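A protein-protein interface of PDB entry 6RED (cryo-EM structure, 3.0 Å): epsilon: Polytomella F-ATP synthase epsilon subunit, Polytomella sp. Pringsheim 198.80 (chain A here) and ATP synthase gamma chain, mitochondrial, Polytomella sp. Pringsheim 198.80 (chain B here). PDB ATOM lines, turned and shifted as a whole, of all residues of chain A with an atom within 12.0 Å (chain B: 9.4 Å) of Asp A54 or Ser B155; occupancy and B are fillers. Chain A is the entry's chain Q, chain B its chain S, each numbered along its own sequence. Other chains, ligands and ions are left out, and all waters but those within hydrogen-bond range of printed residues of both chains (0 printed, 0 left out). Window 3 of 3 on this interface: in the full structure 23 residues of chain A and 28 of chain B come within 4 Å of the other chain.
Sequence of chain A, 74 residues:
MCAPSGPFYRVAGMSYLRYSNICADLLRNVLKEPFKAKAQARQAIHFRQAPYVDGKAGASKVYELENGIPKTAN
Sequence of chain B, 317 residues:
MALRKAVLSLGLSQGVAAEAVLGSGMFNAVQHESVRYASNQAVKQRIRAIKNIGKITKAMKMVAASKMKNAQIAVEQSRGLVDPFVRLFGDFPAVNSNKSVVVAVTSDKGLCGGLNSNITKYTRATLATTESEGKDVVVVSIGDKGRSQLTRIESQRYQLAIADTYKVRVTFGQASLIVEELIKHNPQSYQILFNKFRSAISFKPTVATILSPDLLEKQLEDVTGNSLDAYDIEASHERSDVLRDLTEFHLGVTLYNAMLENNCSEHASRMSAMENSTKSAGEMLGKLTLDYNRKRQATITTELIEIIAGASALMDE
The backbone carbonyl oxygen (O) of Val B139 sits at hydrogen-bond distance from the backbone NH (N) of Gln B159 (3.4 Å).
The side-chain hydroxyl of Thr B151 sits at hydrogen-bond distance from the backbone carbonyl oxygen of Arg B147, at 3.0 Å.
The side-chain amide oxygen (OE1) of Gln B159 lies close to the backbone carbonyl oxygen (O) of Arg B157 (2.9 Å).
OH of Tyr B158 sits close to O of Leu B160 (3.4 Å).
The side-chain hydroxyl (OH) of Tyr A52 lies close to the guanidinium group (NH2) of Arg B147 (3.5 Å).
N of Tyr A52 is in hydrogen-bond range of O of Gln B159 (2.6 Å).
The side-chain hydroxyl (OG) of Ser B155 is in hydrogen-bond range of the backbone carbonyl oxygen (O) of Asp A54 (3.4 Å).
O of Tyr A52 sits close to O of Tyr B158.
O of Ala A50 touches CD1 of Leu B160, at 3.3 Å.
CA of Pro A51 touches O of Gln B159, 3.3 Å away.
Ser B155 touches just one residue of chain A: Asp A54.
No residue of chain B comes within 4 Å of Val A53.
Glu B154 touches none of the printed residues of chain A.
No residue of chain A comes within 4 Å of Gln B156.
Printed residues of chain B within 4 Å of Pro A51: Gln B159.
Printed residues of chain B within 4 Å of Tyr A52: Arg B147 (3.4 Å), Tyr B158 (2.9 Å) and Gln B159 (2.6 Å).
Printed residues of chain A within 4 Å of Arg B147: Tyr A52 (3.4 Å).
The nearest residue of chain A that does not touch Ser B155 is Gly A55 (4.2 Å).
Of the 16 printed residues of chain B, 5 touch a printed residue of chain A.
Of the 10 printed residues of chain A, 4 touch a printed residue of chain B.
Hydrophobic or aromatic side chains of chain A within 4 Å of the printed part of chain B: Tyr A52.
Among the printed residues, 6 pairs touch across the chains.
Among the printed residues, no Asp or Glu carboxylate lies within 4 Å of a Lys or Arg side-chain nitrogen of the other chain.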
ATOM      1  N   ALA A  50      16.538  -6.741   5.628  1.00  0.00           N
ATOM      2  CA  ALA A  50      17.397  -5.609   5.937  1.00  0.00           C
ATOM      3  C   ALA A  50      16.557  -4.381   6.247  1.00  0.00           C
ATOM      4  O   ALA A  50      15.723  -3.987   5.426  1.00  0.00           O
ATOM      5  CB  ALA A  50      18.337  -5.310   4.769  1.00  0.00           C
ATOM      6  N   PRO A  51      16.736  -3.748   7.405  1.00  0.00           N
ATOM      7  CA  PRO A  51      16.076  -2.459   7.650  1.00  0.00           C
ATOM      8  C   PRO A  51      16.771  -1.364   6.855  1.00  0.00           C
ATOM      9  O   PRO A  51      17.999  -1.281   6.845  1.00  0.00           O
ATOM     10  CB  PRO A  51      16.246  -2.247   9.159  1.00  0.00           C
ATOM     11  CG  PRO A  51      16.701  -3.568   9.702  1.00  0.00           C
ATOM     12  CD  PRO A  51      17.448  -4.228   8.597  1.00  0.00           C
ATOM     13  N   TYR A  52      15.989  -0.526   6.184  1.00  0.00           N
ATOM     14  CA  TYR A  52      16.548   0.515   5.323  1.00  0.00           C
ATOM     15  C   TYR A  52      16.354   1.881   5.963  1.00  0.00           C
ATOM     16  O   TYR A  52      15.239   2.398   6.044  1.00  0.00           O
ATOM     17  CB  TYR A  52      15.952   0.441   3.924  1.00  0.00           C
ATOM     18  CG  TYR A  52      16.881  -0.283   2.983  1.00  0.00           C
ATOM     19  CD1 TYR A  52      17.752   0.424   2.162  1.00  0.00           C
ATOM     20  CD2 TYR A  52      16.952  -1.664   2.975  1.00  0.00           C
ATOM     21  CE1 TYR A  52      18.626  -0.229   1.319  1.00  0.00           C
ATOM     22  CE2 TYR A  52      17.832  -2.323   2.145  1.00  0.00           C
ATOM     23  CZ  TYR A  52      18.661  -1.602   1.315  1.00  0.00           C
ATOM     24  OH  TYR A  52      19.533  -2.258   0.479  1.00  0.00           O
ATOM     25  N   VAL A  53      17.468   2.469   6.402  1.00  0.00           N
ATOM     26  CA  VAL A  53      17.416   3.710   7.163  1.00  0.00           C
ATOM     27  C   VAL A  53      17.142   4.901   6.244  1.00  0.00           C
ATOM     28  O   VAL A  53      16.146   5.614   6.415  1.00  0.00           O
ATOM     29  CB  VAL A  53      18.706   3.875   7.993  1.00  0.00           C
ATOM     30  CG1 VAL A  53      18.592   3.077   9.279  1.00  0.00           C
ATOM     31  CG2 VAL A  53      19.933   3.357   7.232  1.00  0.00           C
ATOM     32  N   ASP A  54      18.014   5.141   5.259  1.00  0.00           N
ATOM     33  CA  ASP A  54      17.796   6.193   4.275  1.00  0.00           C
ATOM     34  C   ASP A  54      18.248   5.761   2.889  1.00  0.00           C
ATOM     35  O   ASP A  54      18.560   6.607   2.043  1.00  0.00           O
ATOM     36  CB  ASP A  54      18.517   7.475   4.676  1.00  0.00           C
ATOM     37  CG  ASP A  54      19.887   7.207   5.257  1.00  0.00           C
ATOM     38  OD1 ASP A  54      20.523   8.167   5.739  1.00  0.00           O
ATOM     39  OD2 ASP A  54      20.326   6.037   5.235  1.00  0.00           O
ATOM     40  N   GLY A  55      18.282   4.459   2.635  1.00  0.00           N
ATOM     41  CA  GLY A  55      18.842   3.953   1.402  1.00  0.00           C
ATOM     42  C   GLY A  55      20.079   3.121   1.662  1.00  0.00           C
ATOM     43  O   GLY A  55      20.885   2.897   0.755  1.00  0.00           O
ATOM     44  N   LYS A  56      20.256   2.679   2.906  1.00  0.00           N
ATOM     45  CA  LYS A  56      21.370   1.822   3.295  1.00  0.00           C
ATOM     46  C   LYS A  56      20.843   0.692   4.165  1.00  0.00           C
ATOM     47  O   LYS A  56      19.921   0.897   4.961  1.00  0.00           O
ATOM     48  CB  LYS A  56      22.453   2.616   4.032  1.00  0.00           C
ATOM     49  CG  LYS A  56      23.202   3.601   3.135  1.00  0.00           C
ATOM     50  CD  LYS A  56      24.231   4.412   3.895  1.00  0.00           C
ATOM     51  CE  LYS A  56      24.899   5.418   2.988  1.00  0.00           C
ATOM     52  NZ  LYS A  56      25.850   6.263   3.749  1.00  0.00           N
ATOM     53  N   ALA A  57      21.420  -0.498   4.003  1.00  0.00           N
ATOM     54  CA  ALA A  57      20.870  -1.696   4.633  1.00  0.00           C
ATOM     55  C   ALA A  57      21.453  -1.940   6.019  1.00  0.00           C
ATOM     56  O   ALA A  57      20.731  -1.964   7.019  1.00  0.00           O
ATOM     57  CB  ALA A  57      21.118  -2.909   3.734  1.00  0.00           C
ATOM     58  N   GLY A  58      22.762  -2.116   6.099  1.00  0.00           N
ATOM     59  CA  GLY A  58      23.380  -2.630   7.303  1.00  0.00           C
ATOM     60  C   GLY A  58      24.255  -3.800   6.913  1.00  0.00           C
ATOM     61  O   GLY A  58      25.221  -3.619   6.167  1.00  0.00           O
ATOM     62  N   ALA A  59      23.953  -5.002   7.406  1.00  0.00           N
ATOM     63  CA  ALA A  59      24.414  -6.209   6.726  1.00  0.00           C
ATOM     64  C   ALA A  59      23.236  -7.049   6.248  1.00  0.00           C
ATOM     65  O   ALA A  59      22.970  -7.073   5.043  1.00  0.00           O
ATOM     66  CB  ALA A  59      25.336  -7.010   7.646  1.00  0.00           C
ATOM     67  N   LEU B 127      -0.130   4.282  -4.577  1.00  0.00           N
ATOM     68  CA  LEU B 127       0.427   4.921  -3.398  1.00  0.00           C
ATOM     69  C   LEU B 127       0.209   6.425  -3.436  1.00  0.00           C
ATOM     70  O   LEU B 127       0.121   7.071  -2.392  1.00  0.00           O
ATOM     71  CB  LEU B 127       1.906   4.562  -3.290  1.00  0.00           C
ATOM     72  CG  LEU B 127       2.682   4.963  -2.049  1.00  0.00           C
ATOM     73  CD1 LEU B 127       1.880   4.588  -0.850  1.00  0.00           C
ATOM     74  CD2 LEU B 127       3.993   4.222  -2.035  1.00  0.00           C
ATOM     75  N   VAL B 137       3.607   6.725   5.501  1.00  0.00           N
ATOM     76  CA  VAL B 137       3.690   5.564   4.618  1.00  0.00           C
ATOM     77  C   VAL B 137       5.047   4.904   4.817  1.00  0.00           C
ATOM     78  O   VAL B 137       6.082   5.572   4.736  1.00  0.00           O
ATOM     79  CB  VAL B 137       3.493   5.939   3.132  1.00  0.00           C
ATOM     80  CG1 VAL B 137       3.832   4.772   2.254  1.00  0.00           C
ATOM     81  CG2 VAL B 137       2.064   6.347   2.841  1.00  0.00           C
ATOM     82  N   VAL B 139       7.160   1.871   2.981  1.00  0.00           N
ATOM     83  CA  VAL B 139       7.166   1.052   1.773  1.00  0.00           C
ATOM     84  C   VAL B 139       8.146  -0.095   1.977  1.00  0.00           C
ATOM     85  O   VAL B 139       9.296   0.120   2.374  1.00  0.00           O
ATOM     86  CB  VAL B 139       7.515   1.871   0.525  1.00  0.00           C
ATOM     87  CG1 VAL B 139       7.220   1.068  -0.710  1.00  0.00           C
ATOM     88  CG2 VAL B 139       6.717   3.142   0.507  1.00  0.00           C
ATOM     89  N   ARG B 147      14.105  -3.845  -4.263  1.00  0.00           N
ATOM     90  CA  ARG B 147      14.986  -2.880  -3.621  1.00  0.00           C
ATOM     91  C   ARG B 147      15.856  -2.148  -4.629  1.00  0.00           C
ATOM     92  O   ARG B 147      16.302  -1.034  -4.345  1.00  0.00           O
ATOM     93  CB  ARG B 147      15.857  -3.558  -2.555  1.00  0.00           C
ATOM     94  CG  ARG B 147      17.294  -3.855  -2.959  1.00  0.00           C
ATOM     95  CD  ARG B 147      18.136  -4.320  -1.797  1.00  0.00           C
ATOM     96  NE  ARG B 147      19.280  -5.106  -2.252  1.00  0.00           N
ATOM     97  CZ  ARG B 147      20.430  -4.588  -2.670  1.00  0.00           C
ATOM     98  NH1 ARG B 147      21.413  -5.380  -3.065  1.00  0.00           N
ATOM     99  NH2 ARG B 147      20.600  -3.275  -2.687  1.00  0.00           N
ATOM    100  N   GLN B 149      14.605  -1.088  -7.392  1.00  0.00           N
ATOM    101  CA  GLN B 149      13.679  -0.254  -8.126  1.00  0.00           C
ATOM    102  C   GLN B 149      12.888   0.690  -7.248  1.00  0.00           C
ATOM    103  O   GLN B 149      12.279   1.625  -7.778  1.00  0.00           O
ATOM    104  CB  GLN B 149      12.695  -1.117  -8.929  1.00  0.00           C
ATOM    105  CG  GLN B 149      13.309  -1.715 -10.168  1.00  0.00           C
ATOM    106  CD  GLN B 149      12.302  -2.437 -11.029  1.00  0.00           C
ATOM    107  OE1 GLN B 149      11.100  -2.339 -10.808  1.00  0.00           O
ATOM    108  NE2 GLN B 149      12.789  -3.178 -12.020  1.00  0.00           N
ATOM    109  N   LEU B 150      12.865   0.472  -5.938  1.00  0.00           N
ATOM    110  CA  LEU B 150      12.044   1.274  -5.041  1.00  0.00           C
ATOM    111  C   LEU B 150      12.842   2.261  -4.218  1.00  0.00           C
ATOM    112  O   LEU B 150      12.282   3.265  -3.771  1.00  0.00           O
ATOM    113  CB  LEU B 150      11.243   0.375  -4.101  1.00  0.00           C
ATOM    114  CG  LEU B 150       9.970  -0.251  -4.669  1.00  0.00           C
ATOM    115  CD1 LEU B 150       9.313  -1.078  -3.607  1.00  0.00           C
ATOM    116  CD2 LEU B 150       9.002   0.797  -5.170  1.00  0.00           C
ATOM    117  N   THR B 151      14.132   2.015  -4.010  1.00  0.00           N
ATOM    118  CA  THR B 151      14.986   2.943  -3.285  1.00  0.00           C
ATOM    119  C   THR B 151      15.464   4.104  -4.136  1.00  0.00           C
ATOM    120  O   THR B 151      16.209   4.948  -3.635  1.00  0.00           O
ATOM    121  CB  THR B 151      16.195   2.219  -2.695  1.00  0.00           C
ATOM    122  OG1 THR B 151      17.077   1.813  -3.748  1.00  0.00           O
ATOM    123  CG2 THR B 151      15.766   1.029  -1.882  1.00  0.00           C
ATOM    124  N   ARG B 152      15.067   4.168  -5.402  1.00  0.00           N
ATOM    125  CA  ARG B 152      15.295   5.353  -6.207  1.00  0.00           C
ATOM    126  C   ARG B 152      14.022   6.123  -6.505  1.00  0.00           C
ATOM    127  O   ARG B 152      14.110   7.277  -6.930  1.00  0.00           O
ATOM    128  CB  ARG B 152      15.973   4.988  -7.530  1.00  0.00           C
ATOM    129  CG  ARG B 152      15.119   4.162  -8.463  1.00  0.00           C
ATOM    130  CD  ARG B 152      15.977   3.418  -9.481  1.00  0.00           C
ATOM    131  NE  ARG B 152      16.780   2.358  -8.870  1.00  0.00           N
ATOM    132  CZ  ARG B 152      18.090   2.439  -8.662  1.00  0.00           C
ATOM    133  NH1 ARG B 152      18.742   1.433  -8.097  1.00  0.00           N
ATOM    134  NH2 ARG B 152      18.748   3.531  -9.016  1.00  0.00           N
ATOM    135  N   ILE B 153      12.850   5.538  -6.279  1.00  0.00           N
ATOM    136  CA  ILE B 153      11.589   6.180  -6.607  1.00  0.00           C
ATOM    137  C   ILE B 153      10.852   6.653  -5.357  1.00  0.00           C
ATOM    138  O   ILE B 153      10.190   7.693  -5.388  1.00  0.00           O
ATOM    139  CB  ILE B 153      10.708   5.255  -7.481  1.00  0.00           C
ATOM    140  CG1 ILE B 153       9.551   6.032  -8.093  1.00  0.00           C
ATOM    141  CG2 ILE B 153      10.249   4.008  -6.754  1.00  0.00           C
ATOM    142  CD1 ILE B 153       9.976   6.888  -9.262  1.00  0.00           C
ATOM    143  N   GLU B 154      10.969   5.911  -4.224  1.00  0.00           N
ATOM    144  CA  GLU B 154      10.572   6.374  -2.888  1.00  0.00           C
ATOM    145  C   GLU B 154      11.650   5.918  -1.913  1.00  0.00           C
ATOM    146  O   GLU B 154      11.549   4.853  -1.305  1.00  0.00           O
ATOM    147  CB  GLU B 154       9.198   5.863  -2.454  1.00  0.00           C
ATOM    148  CG  GLU B 154       8.024   6.492  -3.171  1.00  0.00           C
ATOM    149  CD  GLU B 154       7.558   5.679  -4.347  1.00  0.00           C
ATOM    150  OE1 GLU B 154       8.004   4.527  -4.471  1.00  0.00           O
ATOM    151  OE2 GLU B 154       6.755   6.193  -5.152  1.00  0.00           O
ATOM    152  N   SER B 155      12.681   6.739  -1.750  1.00  0.00           N
ATOM    153  CA  SER B 155      13.700   6.479  -0.747  1.00  0.00           C
ATOM    154  C   SER B 155      13.389   7.147   0.579  1.00  0.00           C
ATOM    155  O   SER B 155      14.020   6.817   1.589  1.00  0.00           O
ATOM    156  CB  SER B 155      15.067   6.953  -1.236  1.00  0.00           C
ATOM    157  OG  SER B 155      16.073   6.674  -0.280  1.00  0.00           O
ATOM    158  N   GLN B 156      12.438   8.083   0.592  1.00  0.00           N
ATOM    159  CA  GLN B 156      12.021   8.735   1.824  1.00  0.00           C
ATOM    160  C   GLN B 156      11.206   7.815   2.709  1.00  0.00           C
ATOM    161  O   GLN B 156      11.150   8.031   3.922  1.00  0.00           O
ATOM    162  CB  GLN B 156      11.180   9.977   1.513  1.00  0.00           C
ATOM    163  CG  GLN B 156      11.785  10.950   0.514  1.00  0.00           C
ATOM    164  CD  GLN B 156      13.167  11.431   0.900  1.00  0.00           C
ATOM    165  OE1 GLN B 156      14.107  11.349   0.110  1.00  0.00           O
ATOM    166  NE2 GLN B 156      13.294  11.954   2.111  1.00  0.00           N
ATOM    167  N   ARG B 157      10.587   6.783   2.132  1.00  0.00           N
ATOM    168  CA  ARG B 157       9.568   6.007   2.822  1.00  0.00           C
ATOM    169  C   ARG B 157       9.937   4.531   2.916  1.00  0.00           C
ATOM    170  O   ARG B 157       9.128   3.726   3.374  1.00  0.00           O
ATOM    171  CB  ARG B 157       8.220   6.178   2.116  1.00  0.00           C
ATOM    172  CG  ARG B 157       7.782   7.624   2.017  1.00  0.00           C
ATOM    173  CD  ARG B 157       6.371   7.787   1.498  1.00  0.00           C
ATOM    174  NE  ARG B 157       6.250   7.595   0.059  1.00  0.00           N
ATOM    175  CZ  ARG B 157       5.098   7.700  -0.594  1.00  0.00           C
ATOM    176  NH1 ARG B 157       5.048   7.513  -1.902  1.00  0.00           N
ATOM    177  NH2 ARG B 157       3.992   7.999   0.072  1.00  0.00           N
ATOM    178  N   TYR B 158      11.148   4.170   2.518  1.00  0.00           N
ATOM    179  CA  TYR B 158      11.549   2.779   2.333  1.00  0.00           C
ATOM    180  C   TYR B 158      12.302   2.316   3.575  1.00  0.00           C
ATOM    181  O   TYR B 158      13.456   2.691   3.786  1.00  0.00           O
ATOM    182  CB  TYR B 158      12.408   2.659   1.081  1.00  0.00           C
ATOM    183  CG  TYR B 158      12.637   1.253   0.604  1.00  0.00           C
ATOM    184  CD1 TYR B 158      13.713   0.513   1.068  1.00  0.00           C
ATOM    185  CD2 TYR B 158      11.795   0.673  -0.325  1.00  0.00           C
ATOM    186  CE1 TYR B 158      13.929  -0.763   0.636  1.00  0.00           C
ATOM    187  CE2 TYR B 158      12.009  -0.602  -0.762  1.00  0.00           C
ATOM    188  CZ  TYR B 158      13.075  -1.309  -0.278  1.00  0.00           C
ATOM    189  OH  TYR B 158      13.293  -2.582  -0.717  1.00  0.00           O
ATOM    190  N   GLN B 159      11.653   1.484   4.392  1.00  0.00           N
ATOM    191  CA  GLN B 159      12.254   1.002   5.629  1.00  0.00           C
ATOM    192  C   GLN B 159      12.693  -0.451   5.592  1.00  0.00           C
ATOM    193  O   GLN B 159      13.449  -0.862   6.474  1.00  0.00           O
ATOM    194  CB  GLN B 159      11.292   1.165   6.815  1.00  0.00           C
ATOM    195  CG  GLN B 159      11.393   2.453   7.606  1.00  0.00           C
ATOM    196  CD  GLN B 159      10.487   3.540   7.090  1.00  0.00           C
ATOM    197  OE1 GLN B 159       9.649   3.311   6.226  1.00  0.00           O
ATOM    198  NE2 GLN B 159      10.633   4.733   7.639  1.00  0.00           N
ATOM    199  N   LEU B 160      12.246  -1.243   4.622  1.00  0.00           N
ATOM    200  CA  LEU B 160      12.467  -2.678   4.708  1.00  0.00           C
ATOM    201  C   LEU B 160      12.652  -3.272   3.324  1.00  0.00           C
ATOM    202  O   LEU B 160      11.966  -2.891   2.375  1.00  0.00           O
ATOM    203  CB  LEU B 160      11.304  -3.366   5.416  1.00  0.00           C
ATOM    204  CG  LEU B 160      11.489  -4.798   5.893  1.00  0.00           C
ATOM    205  CD1 LEU B 160      12.781  -4.939   6.651  1.00  0.00           C
ATOM    206  CD2 LEU B 160      10.330  -5.180   6.769  1.00  0.00           C
